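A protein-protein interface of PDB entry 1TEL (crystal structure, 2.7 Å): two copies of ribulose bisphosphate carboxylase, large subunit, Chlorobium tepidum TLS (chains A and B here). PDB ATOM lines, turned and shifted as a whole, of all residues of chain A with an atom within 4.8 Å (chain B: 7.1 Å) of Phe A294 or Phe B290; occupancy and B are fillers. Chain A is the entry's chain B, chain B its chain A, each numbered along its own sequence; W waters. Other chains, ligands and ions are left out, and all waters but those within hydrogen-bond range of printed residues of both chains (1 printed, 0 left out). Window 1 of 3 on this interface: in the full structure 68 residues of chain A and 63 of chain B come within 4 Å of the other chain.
The guanidinium group of Arg A296 is in hydrogen-bond range of the backbone carbonyl oxygen of Tyr B122 (2.8 Å). OH of Tyr A300 sits at hydrogen-bond distance from O of Ala B292 (2.9 Å). The backbone carbonyl oxygen (O) of Ala A292 sits at hydrogen-bond distance from the side-chain hydroxyl (OH) of Tyr B300, at 3.0 Å. The side-chain hydroxyl (OH) of Tyr B300 lies close to the guanidinium group (NE) of Arg A296, at 3.3 Å.
Cys A117 touches Phe B290. Gly A118 touches Pro B289. Gly A118 touches Phe B290. Phe A290 touches Phe B294. Tyr B122 touches Ala A292 (CB to CB, 3.6 Å). CA of Gly B301 touches O of Ser A293, 3.99 Å away. Phe A294 touches Phe B290. Phe A294 touches Phe B294 (CB to CB, 3.8 Å). Tyr A300 touches Ser B293. Gly A301 touches Ser B293.
The side-chain hydroxyl (OH) of Tyr B122 sits at hydrogen-bond distance from the backbone carbonyl oxygen (O) of Gly B301 (2.8 Å). O of Phe B290 sits at hydrogen-bond distance from OG of Ser B293 (2.7 Å). The backbone carbonyl oxygen (O) of Leu A113 sits close to the side-chain sulfur (SG) of Cys A117, at 3.5 Å. O of Phe A290 lies within hydrogen-bond range of OG of Ser A293, at 2.8 Å. The backbone carbonyl oxygen (O) of Phe A294 is in hydrogen-bond range of the backbone NH (N) of Ile A302 (2.8 Å).
Water W1 bridges the backbone carbonyl oxygen (O) of Ser A293 (2.8 Å) and the backbone carbonyl oxygen (O) of Ser B293 (2.9 Å).
Of the 16 printed residues of chain B, 9 touch a printed residue of chain A. Hydrophobic or aromatic side chains of chain B that line the printed part of chain A: Tyr B122, Pro B267, Pro B289, Phe B290, Ala B292, Phe B294 and Tyr B300. Among the printed residues, 20 pairs touch across the chains.
Ala A292 touches Tyr B300, and with the chains exchanged Tyr A300 touches Ala B292. Ser A293 touches Tyr B300, and with the chains exchanged Tyr A300 touches Ser B293. Ser A293 touches Gly B301, and with the chains exchanged Gly A301 touches Ser B293. Phe B294 touches its own counterpart, Phe A294. 10 positions are printed for both chains. Of the 20 pairs that touch across the chains among the printed residues, 11 have their exchanged pair printed and touching as well.
Of the printed residues of chain B, Phe A290 touches Phe B294 (3.4 Å). Phe A294 touches three residues of chain B. Printed residues of chain A within 4 Å of Tyr B122: Ala A292, Ser A293 and Arg A296. Of chain A, only Cys A117, Gly A118, Phe A294 and Ile A302 come within 4 Å of Phe B290. Printed residues of chain A within 4 Å of Ser B293: Phe A294, Tyr A300 and Gly A301. Ser B295 touches none of the printed residues of chain A. Of the printed residues of chain A, Tyr B300 touches Ala A292 (3.0 Å), Ser A293 (3.6 Å) and Arg A296 (3.3 Å). Of the printed residues of chain A, Gly B301 touches Ser A293 (3.99 Å). Met B307 touches none of the printed residues of chain A. The nearest residue of chain B that does not touch Phe A294 is Tyr B300 (5.0 Å). The nearest residue of chain A that does not touch Phe B290 is Leu A113 (4.2 Å). The nearest printed residue of chain A that does not touch Ala B292 is Gly A118 (5.6 Å).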
ATOM      1  N   LEU A 113     -16.644   0.293 -15.489  1.00  0.00           N
ATOM      2  CA  LEU A 113     -17.642   1.065 -16.205  1.00  0.00           C
ATOM      3  C   LEU A 113     -17.134   1.548 -17.553  1.00  0.00           C
ATOM      4  O   LEU A 113     -17.868   1.528 -18.550  1.00  0.00           O
ATOM      5  CB  LEU A 113     -18.083   2.278 -15.381  1.00  0.00           C
ATOM      6  CG  LEU A 113     -19.190   2.035 -14.355  1.00  0.00           C
ATOM      7  CD1 LEU A 113     -20.359   1.341 -15.033  1.00  0.00           C
ATOM      8  CD2 LEU A 113     -18.679   1.168 -13.237  1.00  0.00           C
ATOM      9  N   CYS A 117     -19.408  -0.385 -20.509  1.00  0.00           N
ATOM     10  CA  CYS A 117     -20.442   0.544 -20.951  1.00  0.00           C
ATOM     11  C   CYS A 117     -19.848   1.924 -21.146  1.00  0.00           C
ATOM     12  O   CYS A 117     -20.355   2.915 -20.632  1.00  0.00           O
ATOM     13  CB  CYS A 117     -21.631   0.577 -19.978  1.00  0.00           C
ATOM     14  SG  CYS A 117     -21.231   0.673 -18.264  1.00  0.00           S
ATOM     15  N   GLY A 118     -18.761   1.962 -21.913  1.00  0.00           N
ATOM     16  CA  GLY A 118     -18.071   3.200 -22.193  1.00  0.00           C
ATOM     17  C   GLY A 118     -18.231   3.603 -23.643  1.00  0.00           C
ATOM     18  O   GLY A 118     -19.325   3.516 -24.196  1.00  0.00           O
ATOM     19  N   LEU A 266     -25.348   6.997  -7.354  1.00  0.00           N
ATOM     20  CA  LEU A 266     -24.736   7.555  -8.547  1.00  0.00           C
ATOM     21  C   LEU A 266     -24.297   9.005  -8.488  1.00  0.00           C
ATOM     22  O   LEU A 266     -23.225   9.342  -8.996  1.00  0.00           O
ATOM     23  CB  LEU A 266     -25.633   7.326  -9.755  1.00  0.00           C
ATOM     24  CG  LEU A 266     -25.336   5.928 -10.274  1.00  0.00           C
ATOM     25  CD1 LEU A 266     -26.101   4.894  -9.471  1.00  0.00           C
ATOM     26  CD2 LEU A 266     -25.707   5.871 -11.720  1.00  0.00           C
ATOM     27  N   PHE A 290     -31.056   9.331 -10.180  1.00  0.00           N
ATOM     28  CA  PHE A 290     -30.268   9.328 -11.411  1.00  0.00           C
ATOM     29  C   PHE A 290     -30.299   8.035 -12.240  1.00  0.00           C
ATOM     30  O   PHE A 290     -30.273   8.084 -13.470  1.00  0.00           O
ATOM     31  CB  PHE A 290     -28.817   9.718 -11.108  1.00  0.00           C
ATOM     32  CG  PHE A 290     -28.009  10.027 -12.334  1.00  0.00           C
ATOM     33  CD1 PHE A 290     -27.363   9.009 -13.037  1.00  0.00           C
ATOM     34  CD2 PHE A 290     -27.916  11.341 -12.809  1.00  0.00           C
ATOM     35  CE1 PHE A 290     -26.633   9.284 -14.198  1.00  0.00           C
ATOM     36  CE2 PHE A 290     -27.185  11.625 -13.975  1.00  0.00           C
ATOM     37  CZ  PHE A 290     -26.541  10.591 -14.671  1.00  0.00           C
ATOM     38  N   ILE A 291     -30.371   6.881 -11.588  1.00  0.00           N
ATOM     39  CA  ILE A 291     -30.386   5.626 -12.331  1.00  0.00           C
ATOM     40  C   ILE A 291     -31.435   5.583 -13.445  1.00  0.00           C
ATOM     41  O   ILE A 291     -31.173   5.055 -14.521  1.00  0.00           O
ATOM     42  CB  ILE A 291     -30.595   4.427 -11.381  1.00  0.00           C
ATOM     43  CG1 ILE A 291     -29.427   4.334 -10.396  1.00  0.00           C
ATOM     44  CG2 ILE A 291     -30.689   3.148 -12.171  1.00  0.00           C
ATOM     45  CD1 ILE A 291     -29.635   3.315  -9.296  1.00  0.00           C
ATOM     46  N   ALA A 292     -32.614   6.145 -13.195  1.00  0.00           N
ATOM     47  CA  ALA A 292     -33.678   6.143 -14.202  1.00  0.00           C
ATOM     48  C   ALA A 292     -33.273   6.758 -15.551  1.00  0.00           C
ATOM     49  O   ALA A 292     -33.763   6.337 -16.604  1.00  0.00           O
ATOM     50  CB  ALA A 292     -34.915   6.855 -13.662  1.00  0.00           C
ATOM     51  N   SER A 293     -32.381   7.742 -15.528  1.00  0.00           N
ATOM     52  CA  SER A 293     -31.954   8.391 -16.759  1.00  0.00           C
ATOM     53  C   SER A 293     -31.399   7.411 -17.798  1.00  0.00           C
ATOM     54  O   SER A 293     -31.510   7.654 -19.005  1.00  0.00           O
ATOM     55  CB  SER A 293     -30.912   9.478 -16.459  1.00  0.00           C
ATOM     56  OG  SER A 293     -29.675   8.930 -16.028  1.00  0.00           O
ATOM     57  N   PHE A 294     -30.818   6.302 -17.339  1.00  0.00           N
ATOM     58  CA  PHE A 294     -30.250   5.330 -18.278  1.00  0.00           C
ATOM     59  C   PHE A 294     -30.770   3.892 -18.163  1.00  0.00           C
ATOM     60  O   PHE A 294     -30.231   2.986 -18.800  1.00  0.00           O
ATOM     61  CB  PHE A 294     -28.708   5.326 -18.184  1.00  0.00           C
ATOM     62  CG  PHE A 294     -28.168   4.993 -16.817  1.00  0.00           C
ATOM     63  CD1 PHE A 294     -27.547   5.972 -16.043  1.00  0.00           C
ATOM     64  CD2 PHE A 294     -28.269   3.694 -16.304  1.00  0.00           C
ATOM     65  CE1 PHE A 294     -27.026   5.667 -14.771  1.00  0.00           C
ATOM     66  CE2 PHE A 294     -27.758   3.373 -15.037  1.00  0.00           C
ATOM     67  CZ  PHE A 294     -27.135   4.359 -14.267  1.00  0.00           C
ATOM     68  N   SER A 295     -31.815   3.672 -17.373  1.00  0.00           N
ATOM     69  CA  SER A 295     -32.337   2.315 -17.224  1.00  0.00           C
ATOM     70  C   SER A 295     -33.820   2.142 -17.560  1.00  0.00           C
ATOM     71  O   SER A 295     -34.360   1.044 -17.419  1.00  0.00           O
ATOM     72  CB  SER A 295     -32.098   1.821 -15.797  1.00  0.00           C
ATOM     73  OG  SER A 295     -32.793   2.624 -14.866  1.00  0.00           O
ATOM     74  N   ARG A 296     -34.471   3.217 -17.994  1.00  0.00           N
ATOM     75  CA  ARG A 296     -35.884   3.152 -18.329  1.00  0.00           C
ATOM     76  C   ARG A 296     -36.162   2.576 -19.711  1.00  0.00           C
ATOM     77  O   ARG A 296     -37.005   1.699 -19.845  1.00  0.00           O
ATOM     78  CB  ARG A 296     -36.541   4.533 -18.207  1.00  0.00           C
ATOM     79  CG  ARG A 296     -38.024   4.522 -18.576  1.00  0.00           C
ATOM     80  CD  ARG A 296     -38.786   5.584 -17.829  1.00  0.00           C
ATOM     81  NE  ARG A 296     -38.640   5.418 -16.388  1.00  0.00           N
ATOM     82  CZ  ARG A 296     -38.998   6.328 -15.484  1.00  0.00           C
ATOM     83  NH1 ARG A 296     -38.821   6.083 -14.190  1.00  0.00           N
ATOM     84  NH2 ARG A 296     -39.530   7.481 -15.874  1.00  0.00           N
ATOM     85  N   TYR A 300     -32.428   0.163 -24.318  1.00  0.00           N
ATOM     86  CA  TYR A 300     -31.258   1.023 -24.370  1.00  0.00           C
ATOM     87  C   TYR A 300     -30.738   1.450 -23.010  1.00  0.00           C
ATOM     88  O   TYR A 300     -31.506   1.685 -22.079  1.00  0.00           O
ATOM     89  CB  TYR A 300     -31.554   2.256 -25.221  1.00  0.00           C
ATOM     90  CG  TYR A 300     -30.325   3.100 -25.503  1.00  0.00           C
ATOM     91  CD1 TYR A 300     -29.990   4.191 -24.693  1.00  0.00           C
ATOM     92  CD2 TYR A 300     -29.459   2.767 -26.548  1.00  0.00           C
ATOM     93  CE1 TYR A 300     -28.811   4.924 -24.917  1.00  0.00           C
ATOM     94  CE2 TYR A 300     -28.286   3.486 -26.782  1.00  0.00           C
ATOM     95  CZ  TYR A 300     -27.962   4.559 -25.966  1.00  0.00           C
ATOM     96  OH  TYR A 300     -26.782   5.241 -26.196  1.00  0.00           O
ATOM     97  N   GLY A 301     -29.414   1.531 -22.908  1.00  0.00           N
ATOM     98  CA  GLY A 301     -28.774   1.950 -21.672  1.00  0.00           C
ATOM     99  C   GLY A 301     -28.174   0.854 -20.802  1.00  0.00           C
ATOM    100  O   GLY A 301     -27.335   0.048 -21.235  1.00  0.00           O
ATOM    101  N   ILE A 302     -28.590   0.838 -19.545  1.00  0.00           N
ATOM    102  CA  ILE A 302     -28.095  -0.154 -18.619  1.00  0.00           C
ATOM    103  C   ILE A 302     -29.274  -0.614 -17.784  1.00  0.00           C
ATOM    104  O   ILE A 302     -30.046   0.202 -17.296  1.00  0.00           O
ATOM    105  CB  ILE A 302     -27.008   0.444 -17.717  1.00  0.00           C
ATOM    106  CG1 ILE A 302     -25.963   1.157 -18.586  1.00  0.00           C
ATOM    107  CG2 ILE A 302     -26.354  -0.659 -16.908  1.00  0.00           C
ATOM    108  CD1 ILE A 302     -24.830   1.806 -17.824  1.00  0.00           C
ATOM    109  N   MET A 307     -26.995  -1.860 -11.819  1.00  0.00           N
ATOM    110  CA  MET A 307     -26.650  -0.840 -10.833  1.00  0.00           C
ATOM    111  C   MET A 307     -26.892  -1.341  -9.398  1.00  0.00           C
ATOM    112  O   MET A 307     -26.184  -0.945  -8.462  1.00  0.00           O
ATOM    113  CB  MET A 307     -27.443   0.451 -11.071  1.00  0.00           C
ATOM    114  CG  MET A 307     -27.069   1.177 -12.345  1.00  0.00           C
ATOM    115  SD  MET A 307     -25.281   1.322 -12.562  1.00  0.00           S
ATOM    116  CE  MET A 307     -24.945   2.584 -11.386  1.00  0.00           C
ATOM    117  N   TYR B 122     -37.691  11.847 -12.545  1.00  0.00           N
ATOM    118  CA  TYR B 122     -38.116  10.744 -13.387  1.00  0.00           C
ATOM    119  C   TYR B 122     -39.256   9.889 -12.863  1.00  0.00           C
ATOM    120  O   TYR B 122     -39.665   8.950 -13.544  1.00  0.00           O
ATOM    121  CB  TYR B 122     -36.917   9.846 -13.705  1.00  0.00           C
ATOM    122  CG  TYR B 122     -35.785  10.560 -14.418  1.00  0.00           C
ATOM    123  CD1 TYR B 122     -34.636  10.959 -13.729  1.00  0.00           C
ATOM    124  CD2 TYR B 122     -35.875  10.862 -15.779  1.00  0.00           C
ATOM    125  CE1 TYR B 122     -33.605  11.648 -14.384  1.00  0.00           C
ATOM    126  CE2 TYR B 122     -34.857  11.545 -16.440  1.00  0.00           C
ATOM    127  CZ  TYR B 122     -33.724  11.940 -15.743  1.00  0.00           C
ATOM    128  OH  TYR B 122     -32.724  12.629 -16.407  1.00  0.00           O
ATOM    129  N   ALA B 265     -14.679  11.067 -16.872  1.00  0.00           N
ATOM    130  CA  ALA B 265     -15.613  11.857 -16.079  1.00  0.00           C
ATOM    131  C   ALA B 265     -16.671  11.139 -15.249  1.00  0.00           C
ATOM    132  O   ALA B 265     -16.612  11.165 -14.024  1.00  0.00           O
ATOM    133  CB  ALA B 265     -16.272  12.878 -16.976  1.00  0.00           C
ATOM    134  N   LEU B 266     -17.643  10.503 -15.894  1.00  0.00           N
ATOM    135  CA  LEU B 266     -18.692   9.836 -15.137  1.00  0.00           C
ATOM    136  C   LEU B 266     -18.322   8.569 -14.386  1.00  0.00           C
ATOM    137  O   LEU B 266     -18.761   8.372 -13.252  1.00  0.00           O
ATOM    138  CB  LEU B 266     -19.899   9.586 -16.024  1.00  0.00           C
ATOM    139  CG  LEU B 266     -20.726  10.872 -16.033  1.00  0.00           C
ATOM    140  CD1 LEU B 266     -20.136  11.869 -17.020  1.00  0.00           C
ATOM    141  CD2 LEU B 266     -22.141  10.537 -16.393  1.00  0.00           C
ATOM    142  N   PRO B 267     -17.531   7.680 -15.002  1.00  0.00           N
ATOM    143  CA  PRO B 267     -17.155   6.455 -14.281  1.00  0.00           C
ATOM    144  C   PRO B 267     -16.497   6.781 -12.920  1.00  0.00           C
ATOM    145  O   PRO B 267     -16.561   5.996 -11.966  1.00  0.00           O
ATOM    146  CB  PRO B 267     -16.191   5.776 -15.255  1.00  0.00           C
ATOM    147  CG  PRO B 267     -16.759   6.155 -16.587  1.00  0.00           C
ATOM    148  CD  PRO B 267     -17.088   7.629 -16.408  1.00  0.00           C
ATOM    149  N   HIS B 287     -12.860  12.592 -20.457  1.00  0.00           N
ATOM    150  CA  HIS B 287     -13.367  11.795 -21.568  1.00  0.00           C
ATOM    151  C   HIS B 287     -14.851  11.517 -21.329  1.00  0.00           C
ATOM    152  O   HIS B 287     -15.333  11.630 -20.197  1.00  0.00           O
ATOM    153  CB  HIS B 287     -12.603  10.486 -21.682  1.00  0.00           C
ATOM    154  CG  HIS B 287     -12.486   9.989 -23.089  1.00  0.00           C
ATOM    155  ND1 HIS B 287     -11.292   9.975 -23.779  1.00  0.00           N
ATOM    156  CD2 HIS B 287     -13.420   9.515 -23.948  1.00  0.00           C
ATOM    157  CE1 HIS B 287     -11.493   9.513 -25.001  1.00  0.00           C
ATOM    158  NE2 HIS B 287     -12.776   9.226 -25.130  1.00  0.00           N
ATOM    159  N   PHE B 288     -15.564  11.121 -22.381  1.00  0.00           N
ATOM    160  CA  PHE B 288     -17.009  10.895 -22.290  1.00  0.00           C
ATOM    161  C   PHE B 288     -17.646   9.506 -22.111  1.00  0.00           C
ATOM    162  O   PHE B 288     -18.846   9.352 -22.364  1.00  0.00           O
ATOM    163  CB  PHE B 288     -17.670  11.545 -23.496  1.00  0.00           C
ATOM    164  CG  PHE B 288     -17.150  11.045 -24.802  1.00  0.00           C
ATOM    165  CD1 PHE B 288     -16.056  11.642 -25.401  1.00  0.00           C
ATOM    166  CD2 PHE B 288     -17.753   9.960 -25.436  1.00  0.00           C
ATOM    167  CE1 PHE B 288     -15.568  11.161 -26.625  1.00  0.00           C
ATOM    168  CE2 PHE B 288     -17.274   9.471 -26.656  1.00  0.00           C
ATOM    169  CZ  PHE B 288     -16.179  10.073 -27.253  1.00  0.00           C
ATOM    170  N   PRO B 289     -16.887   8.486 -21.671  1.00  0.00           N
ATOM    171  CA  PRO B 289     -17.531   7.174 -21.510  1.00  0.00           C
ATOM    172  C   PRO B 289     -18.745   7.244 -20.591  1.00  0.00           C
ATOM    173  O   PRO B 289     -18.791   8.057 -19.671  1.00  0.00           O
ATOM    174  CB  PRO B 289     -16.432   6.309 -20.897  1.00  0.00           C
ATOM    175  CG  PRO B 289     -15.163   6.931 -21.436  1.00  0.00           C
ATOM    176  CD  PRO B 289     -15.452   8.424 -21.332  1.00  0.00           C
ATOM    177  N   PHE B 290     -19.726   6.390 -20.859  1.00  0.00           N
ATOM    178  CA  PHE B 290     -20.943   6.293 -20.058  1.00  0.00           C
ATOM    179  C   PHE B 290     -22.030   7.328 -20.350  1.00  0.00           C
ATOM    180  O   PHE B 290     -23.222   7.019 -20.252  1.00  0.00           O
ATOM    181  CB  PHE B 290     -20.591   6.310 -18.562  1.00  0.00           C
ATOM    182  CG  PHE B 290     -21.740   5.937 -17.663  1.00  0.00           C
ATOM    183  CD1 PHE B 290     -22.659   6.890 -17.245  1.00  0.00           C
ATOM    184  CD2 PHE B 290     -21.924   4.614 -17.266  1.00  0.00           C
ATOM    185  CE1 PHE B 290     -23.746   6.534 -16.447  1.00  0.00           C
ATOM    186  CE2 PHE B 290     -23.017   4.250 -16.463  1.00  0.00           C
ATOM    187  CZ  PHE B 290     -23.928   5.209 -16.055  1.00  0.00           C
ATOM    188  N   ILE B 291     -21.647   8.543 -20.714  1.00  0.00           N
ATOM    189  CA  ILE B 291     -22.654   9.565 -20.981  1.00  0.00           C
ATOM    190  C   ILE B 291     -23.730   9.126 -21.979  1.00  0.00           C
ATOM    191  O   ILE B 291     -24.904   9.445 -21.807  1.00  0.00           O
ATOM    192  CB  ILE B 291     -21.996  10.868 -21.486  1.00  0.00           C
ATOM    193  CG1 ILE B 291     -21.083  11.437 -20.403  1.00  0.00           C
ATOM    194  CG2 ILE B 291     -23.046  11.891 -21.836  1.00  0.00           C
ATOM    195  CD1 ILE B 291     -20.248  12.612 -20.863  1.00  0.00           C
ATOM    196  N   ALA B 292     -23.337   8.387 -23.013  1.00  0.00           N
ATOM    197  CA  ALA B 292     -24.287   7.931 -24.030  1.00  0.00           C
ATOM    198  C   ALA B 292     -25.480   7.142 -23.474  1.00  0.00           C
ATOM    199  O   ALA B 292     -26.576   7.200 -24.024  1.00  0.00           O
ATOM    200  CB  ALA B 292     -23.562   7.099 -25.086  1.00  0.00           C
ATOM    201  N   SER B 293     -25.264   6.407 -22.388  1.00  0.00           N
ATOM    202  CA  SER B 293     -26.330   5.613 -21.783  1.00  0.00           C
ATOM    203  C   SER B 293     -27.567   6.434 -21.428  1.00  0.00           C
ATOM    204  O   SER B 293     -28.678   5.908 -21.429  1.00  0.00           O
ATOM    205  CB  SER B 293     -25.820   4.891 -20.522  1.00  0.00           C
ATOM    206  OG  SER B 293     -25.524   5.796 -19.468  1.00  0.00           O
ATOM    207  N   PHE B 294     -27.385   7.717 -21.127  1.00  0.00           N
ATOM    208  CA  PHE B 294     -28.530   8.557 -20.764  1.00  0.00           C
ATOM    209  C   PHE B 294     -28.740   9.830 -21.589  1.00  0.00           C
ATOM    210  O   PHE B 294     -29.578  10.652 -21.241  1.00  0.00           O
ATOM    211  CB  PHE B 294     -28.471   8.928 -19.270  1.00  0.00           C
ATOM    212  CG  PHE B 294     -27.215   9.672 -18.862  1.00  0.00           C
ATOM    213  CD1 PHE B 294     -26.256   9.056 -18.055  1.00  0.00           C
ATOM    214  CD2 PHE B 294     -26.999  10.993 -19.266  1.00  0.00           C
ATOM    215  CE1 PHE B 294     -25.102   9.744 -17.653  1.00  0.00           C
ATOM    216  CE2 PHE B 294     -25.849  11.689 -18.870  1.00  0.00           C
ATOM    217  CZ  PHE B 294     -24.898  11.064 -18.062  1.00  0.00           C
ATOM    218  N   SER B 295     -27.997   9.990 -22.679  1.00  0.00           N
ATOM    219  CA  SER B 295     -28.129  11.194 -23.509  1.00  0.00           C
ATOM    220  C   SER B 295     -28.448  10.941 -24.991  1.00  0.00           C
ATOM    221  O   SER B 295     -28.542  11.884 -25.783  1.00  0.00           O
ATOM    222  CB  SER B 295     -26.850  12.035 -23.418  1.00  0.00           C
ATOM    223  OG  SER B 295     -25.736  11.334 -23.943  1.00  0.00           O
ATOM    224  N   TYR B 300     -35.492  11.654 -23.908  1.00  0.00           N
ATOM    225  CA  TYR B 300     -35.392  11.085 -22.567  1.00  0.00           C
ATOM    226  C   TYR B 300     -33.979  11.101 -21.990  1.00  0.00           C
ATOM    227  O   TYR B 300     -32.995  10.913 -22.706  1.00  0.00           O
ATOM    228  CB  TYR B 300     -35.939   9.647 -22.559  1.00  0.00           C
ATOM    229  CG  TYR B 300     -36.062   9.052 -21.164  1.00  0.00           C
ATOM    230  CD1 TYR B 300     -35.037   8.274 -20.614  1.00  0.00           C
ATOM    231  CD2 TYR B 300     -37.171   9.339 -20.363  1.00  0.00           C
ATOM    232  CE1 TYR B 300     -35.118   7.802 -19.291  1.00  0.00           C
ATOM    233  CE2 TYR B 300     -37.261   8.878 -19.058  1.00  0.00           C
ATOM    234  CZ  TYR B 300     -36.236   8.114 -18.519  1.00  0.00           C
ATOM    235  OH  TYR B 300     -36.334   7.680 -17.211  1.00  0.00           O
ATOM    236  N   GLY B 301     -33.895  11.339 -20.685  1.00  0.00           N
ATOM    237  CA  GLY B 301     -32.609  11.352 -20.016  1.00  0.00           C
ATOM    238  C   GLY B 301     -32.034  12.722 -19.699  1.00  0.00           C
ATOM    239  O   GLY B 301     -32.669  13.572 -19.062  1.00  0.00           O
ATOM    240  N   MET B 307     -23.899  17.542 -19.372  1.00  0.00           N
ATOM    241  CA  MET B 307     -22.724  16.868 -18.826  1.00  0.00           C
ATOM    242  C   MET B 307     -21.434  17.610 -19.216  1.00  0.00           C
ATOM    243  O   MET B 307     -20.457  17.607 -18.468  1.00  0.00           O
ATOM    244  CB  MET B 307     -22.652  15.409 -19.301  1.00  0.00           C
ATOM    245  CG  MET B 307     -23.742  14.514 -18.746  1.00  0.00           C
ATOM    246  SD  MET B 307     -23.941  14.716 -16.974  1.00  0.00           S
ATOM    247  CE  MET B 307     -22.523  13.883 -16.390  1.00  0.00           C
HETATM  248  O   HOH W   1     -31.539   6.330 -21.437  1.00  0.00           O
